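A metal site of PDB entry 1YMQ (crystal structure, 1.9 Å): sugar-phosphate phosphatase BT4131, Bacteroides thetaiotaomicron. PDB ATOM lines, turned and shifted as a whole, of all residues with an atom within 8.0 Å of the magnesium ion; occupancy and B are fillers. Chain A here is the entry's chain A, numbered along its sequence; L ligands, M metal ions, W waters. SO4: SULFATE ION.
Water W1 bridges OD1 of Asn 214 (2.7 Å) and OD2 of Asp 215 (2.8 Å).
Of the 24 residues printed, 3 come within 4 Å of the magnesium ion.
The nearest printed residue that does not touch the magnesium ion is Asp 215 (4.02 Å).
OD1 of Asp 8 lies close to OG1 of Thr 12.
OD2 of Asp 8 lies within salt-bridge range of NZ of Lys 188.
The backbone NH (N) of Asp 8 lies within hydrogen-bond range of the backbone carbonyl oxygen (O) of Phe 209 (3.2 Å).
The side-chain carboxylate of Asp 215 lies within hydrogen-bond range of the backbone NH of Asp 211 (3.0 Å).
The backbone NH of Asp 211 sits at hydrogen-bond distance from the side-chain hydroxyl of Thr 12, 3.3 Å away.
The magnesium ion is bound by OD1 of Asp 8 (2.2 Å), O of Asp 10 (2.3 Å), O2 of the ligand (2.3 Å), water W1 (2.3 Å), OD1 of Asp 211 (2.3 Å) and water W2 (2.4 Å).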
ATOM      1  N   PHE A   7      23.480  29.454 -15.704  1.00  0.00           N
ATOM      2  CA  PHE A   7      24.213  28.434 -14.955  1.00  0.00           C
ATOM      3  C   PHE A   7      23.956  27.021 -15.421  1.00  0.00           C
ATOM      4  O   PHE A   7      22.805  26.570 -15.479  1.00  0.00           O
ATOM      5  CB  PHE A   7      23.810  28.458 -13.456  1.00  0.00           C
ATOM      6  CG  PHE A   7      24.082  29.736 -12.773  1.00  0.00           C
ATOM      7  CD1 PHE A   7      23.100  30.709 -12.651  1.00  0.00           C
ATOM      8  CD2 PHE A   7      25.358  29.975 -12.198  1.00  0.00           C
ATOM      9  CE1 PHE A   7      23.369  31.933 -11.964  1.00  0.00           C
ATOM     10  CE2 PHE A   7      25.656  31.149 -11.521  1.00  0.00           C
ATOM     11  CZ  PHE A   7      24.683  32.140 -11.402  1.00  0.00           C
ATOM     12  N   ASP A   8      25.031  26.321 -15.673  1.00  0.00           N
ATOM     13  CA  ASP A   8      24.951  24.882 -15.943  1.00  0.00           C
ATOM     14  C   ASP A   8      24.615  24.277 -14.554  1.00  0.00           C
ATOM     15  O   ASP A   8      24.874  24.892 -13.509  1.00  0.00           O
ATOM     16  CB  ASP A   8      26.330  24.394 -16.388  1.00  0.00           C
ATOM     17  CG  ASP A   8      26.414  22.925 -16.377  1.00  0.00           C
ATOM     18  OD1 ASP A   8      27.410  22.430 -15.838  1.00  0.00           O
ATOM     19  OD2 ASP A   8      25.449  22.295 -16.913  1.00  0.00           O
ATOM     20  N   ILE A   9      24.063  23.081 -14.519  1.00  0.00           N
ATOM     21  CA  ILE A   9      23.722  22.501 -13.204  1.00  0.00           C
ATOM     22  C   ILE A   9      24.861  21.669 -12.613  1.00  0.00           C
ATOM     23  O   ILE A   9      25.529  22.095 -11.658  1.00  0.00           O
ATOM     24  CB  ILE A   9      22.473  21.562 -13.298  1.00  0.00           C
ATOM     25  CG1 ILE A   9      21.251  22.387 -13.694  1.00  0.00           C
ATOM     26  CG2 ILE A   9      22.199  20.871 -11.899  1.00  0.00           C
ATOM     27  CD1 ILE A   9      19.913  21.548 -13.949  1.00  0.00           C
ATOM     28  N   ASP A  10      25.095  20.509 -13.201  1.00  0.00           N
ATOM     29  CA  ASP A  10      26.064  19.550 -12.673  1.00  0.00           C
ATOM     30  C   ASP A  10      27.526  19.969 -12.757  1.00  0.00           C
ATOM     31  O   ASP A  10      28.084  20.077 -13.831  1.00  0.00           O
ATOM     32  CB  ASP A  10      25.834  18.174 -13.337  1.00  0.00           C
ATOM     33  CG  ASP A  10      24.417  17.699 -13.170  1.00  0.00           C
ATOM     34  OD1 ASP A  10      23.993  17.431 -12.024  1.00  0.00           O
ATOM     35  OD2 ASP A  10      23.689  17.622 -14.191  1.00  0.00           O
ATOM     36  N   GLY A  11      28.140  20.160 -11.586  1.00  0.00           N
ATOM     37  CA  GLY A  11      29.521  20.603 -11.559  1.00  0.00           C
ATOM     38  C   GLY A  11      29.620  22.142 -11.540  1.00  0.00           C
ATOM     39  O   GLY A  11      30.714  22.676 -11.426  1.00  0.00           O
ATOM     40  N   THR A  12      28.494  22.861 -11.631  1.00  0.00           N
ATOM     41  CA  THR A  12      28.536  24.336 -11.630  1.00  0.00           C
ATOM     42  C   THR A  12      27.705  24.859 -10.451  1.00  0.00           C
ATOM     43  O   THR A  12      28.209  25.579  -9.605  1.00  0.00           O
ATOM     44  CB  THR A  12      28.071  24.843 -12.997  1.00  0.00           C
ATOM     45  OG1 THR A  12      28.991  24.370 -13.994  1.00  0.00           O
ATOM     46  CG2 THR A  12      28.022  26.383 -13.019  1.00  0.00           C
ATOM     47  N   LEU A  13      26.441  24.441 -10.366  1.00  0.00           N
ATOM     48  CA  LEU A  13      25.591  24.744  -9.213  1.00  0.00           C
ATOM     49  C   LEU A  13      25.673  23.587  -8.194  1.00  0.00           C
ATOM     50  O   LEU A  13      25.844  23.782  -6.996  1.00  0.00           O
ATOM     51  CB  LEU A  13      24.119  24.875  -9.648  1.00  0.00           C
ATOM     52  CG  LEU A  13      23.837  26.161 -10.491  1.00  0.00           C
ATOM     53  CD1 LEU A  13      22.439  26.114 -11.102  1.00  0.00           C
ATOM     54  CD2 LEU A  13      23.990  27.401  -9.561  1.00  0.00           C
ATOM     55  N   VAL A  14      25.513  22.357  -8.698  1.00  0.00           N
ATOM     56  CA  VAL A  14      25.451  21.161  -7.827  1.00  0.00           C
ATOM     57  C   VAL A  14      26.748  20.398  -7.891  1.00  0.00           C
ATOM     58  O   VAL A  14      27.226  20.115  -8.969  1.00  0.00           O
ATOM     59  CB  VAL A  14      24.344  20.193  -8.303  1.00  0.00           C
ATOM     60  CG1 VAL A  14      24.215  19.019  -7.359  1.00  0.00           C
ATOM     61  CG2 VAL A  14      22.978  20.949  -8.364  1.00  0.00           C
ATOM     62  N   PHE A  16      29.308  17.352  -7.768  1.00  0.00           N
ATOM     63  CA  PHE A  16      29.274  15.933  -8.128  1.00  0.00           C
ATOM     64  C   PHE A  16      29.724  15.205  -6.852  1.00  0.00           C
ATOM     65  O   PHE A  16      29.329  14.085  -6.601  1.00  0.00           O
ATOM     66  CB  PHE A  16      30.283  15.614  -9.231  1.00  0.00           C
ATOM     67  CG  PHE A  16      29.764  15.815 -10.631  1.00  0.00           C
ATOM     68  CD1 PHE A  16      28.731  15.035 -11.109  1.00  0.00           C
ATOM     69  CD2 PHE A  16      30.307  16.809 -11.440  1.00  0.00           C
ATOM     70  CE1 PHE A  16      28.221  15.248 -12.402  1.00  0.00           C
ATOM     71  CE2 PHE A  16      29.825  17.034 -12.706  1.00  0.00           C
ATOM     72  CZ  PHE A  16      28.766  16.254 -13.203  1.00  0.00           C
ATOM     73  N   ALA A  42      20.945  26.384 -17.600  1.00  0.00           N
ATOM     74  CA  ALA A  42      21.328  26.016 -18.971  1.00  0.00           C
ATOM     75  C   ALA A  42      21.984  24.656 -18.780  1.00  0.00           C
ATOM     76  O   ALA A  42      23.170  24.554 -18.443  1.00  0.00           O
ATOM     77  CB  ALA A  42      22.318  27.068 -19.608  1.00  0.00           C
ATOM     78  N   THR A  43      21.181  23.627 -19.004  1.00  0.00           N
ATOM     79  CA  THR A  43      21.583  22.247 -18.758  1.00  0.00           C
ATOM     80  C   THR A  43      21.364  21.285 -19.939  1.00  0.00           C
ATOM     81  O   THR A  43      20.541  21.538 -20.823  1.00  0.00           O
ATOM     82  CB  THR A  43      20.808  21.709 -17.511  1.00  0.00           C
ATOM     83  OG1 THR A  43      21.295  20.389 -17.173  1.00  0.00           O
ATOM     84  CG2 THR A  43      19.283  21.693 -17.746  1.00  0.00           C
ATOM     85  N   GLY A  44      22.184  20.216 -19.970  1.00  0.00           N
ATOM     86  CA  GLY A  44      22.014  19.196 -20.991  1.00  0.00           C
ATOM     87  C   GLY A  44      20.912  18.281 -20.501  1.00  0.00           C
ATOM     88  O   GLY A  44      20.405  17.451 -21.261  1.00  0.00           O
ATOM     89  N   TRP A 174      30.573  16.076 -21.631  1.00  0.00           N
ATOM     90  CA  TRP A 174      31.305  16.523 -20.470  1.00  0.00           C
ATOM     91  C   TRP A 174      31.785  15.267 -19.732  1.00  0.00           C
ATOM     92  O   TRP A 174      32.602  15.340 -18.816  1.00  0.00           O
ATOM     93  CB  TRP A 174      30.405  17.377 -19.589  1.00  0.00           C
ATOM     94  CG  TRP A 174      29.169  16.692 -19.149  1.00  0.00           C
ATOM     95  CD1 TRP A 174      27.948  16.752 -19.731  1.00  0.00           C
ATOM     96  CD2 TRP A 174      29.043  15.864 -18.004  1.00  0.00           C
ATOM     97  NE1 TRP A 174      27.037  16.013 -19.002  1.00  0.00           N
ATOM     98  CE2 TRP A 174      27.690  15.444 -17.933  1.00  0.00           C
ATOM     99  CE3 TRP A 174      29.929  15.437 -17.008  1.00  0.00           C
ATOM    100  CZ2 TRP A 174      27.220  14.613 -16.925  1.00  0.00           C
ATOM    101  CZ3 TRP A 174      29.462  14.602 -16.009  1.00  0.00           C
ATOM    102  CH2 TRP A 174      28.122  14.205 -15.973  1.00  0.00           C
ATOM    103  N   LYS A 188      23.828  25.312 -25.835  1.00  0.00           N
ATOM    104  CA  LYS A 188      23.428  26.325 -24.830  1.00  0.00           C
ATOM    105  C   LYS A 188      23.525  27.739 -25.346  1.00  0.00           C
ATOM    106  O   LYS A 188      22.800  28.611 -24.875  1.00  0.00           O
ATOM    107  CB  LYS A 188      24.247  26.111 -23.548  1.00  0.00           C
ATOM    108  CG  LYS A 188      23.841  24.768 -22.858  1.00  0.00           C
ATOM    109  CD  LYS A 188      24.796  24.466 -21.632  1.00  0.00           C
ATOM    110  CE  LYS A 188      24.477  23.026 -21.062  1.00  0.00           C
ATOM    111  NZ  LYS A 188      25.178  22.853 -19.761  1.00  0.00           N
ATOM    112  N   PHE A 209      28.149  30.400 -16.757  1.00  0.00           N
ATOM    113  CA  PHE A 209      29.012  29.667 -15.839  1.00  0.00           C
ATOM    114  C   PHE A 209      28.909  28.200 -16.226  1.00  0.00           C
ATOM    115  O   PHE A 209      27.816  27.672 -16.364  1.00  0.00           O
ATOM    116  CB  PHE A 209      28.569  29.796 -14.383  1.00  0.00           C
ATOM    117  CG  PHE A 209      28.434  31.210 -13.874  1.00  0.00           C
ATOM    118  CD1 PHE A 209      27.369  32.019 -14.298  1.00  0.00           C
ATOM    119  CD2 PHE A 209      29.394  31.725 -12.993  1.00  0.00           C
ATOM    120  CE1 PHE A 209      27.256  33.345 -13.855  1.00  0.00           C
ATOM    121  CE2 PHE A 209      29.308  33.060 -12.545  1.00  0.00           C
ATOM    122  CZ  PHE A 209      28.254  33.853 -12.961  1.00  0.00           C
ATOM    123  N   GLY A 210      30.057  27.550 -16.343  1.00  0.00           N
ATOM    124  CA  GLY A 210      30.057  26.133 -16.726  1.00  0.00           C
ATOM    125  C   GLY A 210      31.318  25.383 -16.373  1.00  0.00           C
ATOM    126  O   GLY A 210      32.363  25.986 -16.120  1.00  0.00           O
ATOM    127  N   ASP A 211      31.240  24.037 -16.400  1.00  0.00           N
ATOM    128  CA  ASP A 211      32.415  23.211 -16.091  1.00  0.00           C
ATOM    129  C   ASP A 211      32.675  22.126 -17.147  1.00  0.00           C
ATOM    130  O   ASP A 211      33.636  21.426 -17.031  1.00  0.00           O
ATOM    131  CB  ASP A 211      32.193  22.423 -14.780  1.00  0.00           C
ATOM    132  CG  ASP A 211      31.194  21.321 -14.950  1.00  0.00           C
ATOM    133  OD1 ASP A 211      30.114  21.585 -15.510  1.00  0.00           O
ATOM    134  OD2 ASP A 211      31.484  20.196 -14.519  1.00  0.00           O
ATOM    135  N   GLY A 212      31.815  22.014 -18.172  1.00  0.00           N
ATOM    136  CA  GLY A 212      31.943  20.923 -19.111  1.00  0.00           C
ATOM    137  C   GLY A 212      32.018  21.263 -20.581  1.00  0.00           C
ATOM    138  O   GLY A 212      31.777  22.390 -20.987  1.00  0.00           O
ATOM    139  N   GLY A 213      32.356  20.244 -21.385  1.00  0.00           N
ATOM    140  CA  GLY A 213      32.500  20.465 -22.812  1.00  0.00           C
ATOM    141  C   GLY A 213      31.244  21.053 -23.472  1.00  0.00           C
ATOM    142  O   GLY A 213      31.387  21.887 -24.366  1.00  0.00           O
ATOM    143  N   ASN A 214      30.054  20.649 -23.037  1.00  0.00           N
ATOM    144  CA  ASN A 214      28.822  21.158 -23.613  1.00  0.00           C
ATOM    145  C   ASN A 214      28.528  22.621 -23.174  1.00  0.00           C
ATOM    146  O   ASN A 214      27.508  23.174 -23.564  1.00  0.00           O
ATOM    147  CB  ASN A 214      27.602  20.239 -23.327  1.00  0.00           C
ATOM    148  CG  ASN A 214      27.286  20.103 -21.844  1.00  0.00           C
ATOM    149  OD1 ASN A 214      28.176  20.128 -20.990  1.00  0.00           O
ATOM    150  ND2 ASN A 214      26.005  19.909 -21.528  1.00  0.00           N
ATOM    151  N   ASP A 215      29.460  23.231 -22.436  1.00  0.00           N
ATOM    152  CA  ASP A 215      29.323  24.615 -21.984  1.00  0.00           C
ATOM    153  C   ASP A 215      30.226  25.528 -22.788  1.00  0.00           C
ATOM    154  O   ASP A 215      30.117  26.732 -22.685  1.00  0.00           O
ATOM    155  CB  ASP A 215      29.689  24.791 -20.479  1.00  0.00           C
ATOM    156  CG  ASP A 215      28.778  24.012 -19.566  1.00  0.00           C
ATOM    157  OD1 ASP A 215      27.564  24.032 -19.865  1.00  0.00           O
ATOM    158  OD2 ASP A 215      29.245  23.393 -18.554  1.00  0.00           O
ATOM    159  N   MET A 218      28.436  28.338 -24.796  1.00  0.00           N
ATOM    160  CA  MET A 218      27.851  29.480 -24.085  1.00  0.00           C
ATOM    161  C   MET A 218      28.895  30.265 -23.313  1.00  0.00           C
ATOM    162  O   MET A 218      28.679  31.431 -22.992  1.00  0.00           O
ATOM    163  CB  MET A 218      26.692  29.045 -23.157  1.00  0.00           C
ATOM    164  CG  MET A 218      27.089  28.235 -21.927  1.00  0.00           C
ATOM    165  SD  MET A 218      25.682  28.216 -20.737  1.00  0.00           S
ATOM    166  CE  MET A 218      26.452  27.407 -19.360  1.00  0.00           C
ATOM    167  N   MET A 228      34.409  26.885 -14.123  1.00  0.00           N
ATOM    168  CA  MET A 228      34.624  26.400 -12.779  1.00  0.00           C
ATOM    169  C   MET A 228      36.093  25.965 -12.643  1.00  0.00           C
ATOM    170  O   MET A 228      36.698  25.486 -13.619  1.00  0.00           O
ATOM    171  CB  MET A 228      33.683  25.227 -12.481  1.00  0.00           C
ATOM    172  CG  MET A 228      32.142  25.635 -12.585  1.00  0.00           C
ATOM    173  SD  MET A 228      31.758  27.170 -11.674  1.00  0.00           S
ATOM    174  CE  MET A 228      31.912  26.636  -9.890  1.00  0.00           C
ATOM    175  N   GLN A 230      37.560  23.457 -11.460  1.00  0.00           N
ATOM    176  CA  GLN A 230      37.931  22.086 -11.700  1.00  0.00           C
ATOM    177  C   GLN A 230      37.598  21.620 -13.144  1.00  0.00           C
ATOM    178  O   GLN A 230      37.647  20.447 -13.466  1.00  0.00           O
ATOM    179  CB  GLN A 230      37.235  21.194 -10.662  1.00  0.00           C
ATOM    180  CG  GLN A 230      35.726  20.763 -10.965  1.00  0.00           C
ATOM    181  CD  GLN A 230      34.657  21.908 -10.755  1.00  0.00           C
ATOM    182  OE1 GLN A 230      34.940  22.958 -10.121  1.00  0.00           O
ATOM    183  NE2 GLN A 230      33.452  21.692 -11.306  1.00  0.00           N
HETATM  184  S   SO4 L   1      24.691  19.598 -17.078  1.00  0.00           S
HETATM  185  O1  SO4 L   1      23.859  20.498 -16.257  1.00  0.00           O
HETATM  186  O2  SO4 L   1      26.091  19.549 -16.493  1.00  0.00           O
HETATM  187  O3  SO4 L   1      24.064  18.227 -17.024  1.00  0.00           O
HETATM  188  O4  SO4 L   1      24.818  19.994 -18.528  1.00  0.00           O
HETATM  189 MG    MG M   1      28.191  20.409 -16.076  1.00  0.00          MG
HETATM  190  O   HOH W   1      28.526  20.698 -18.354  1.00  0.00           O
HETATM  191  O   HOH W   2      29.752  18.649 -15.991  1.00  0.00           O
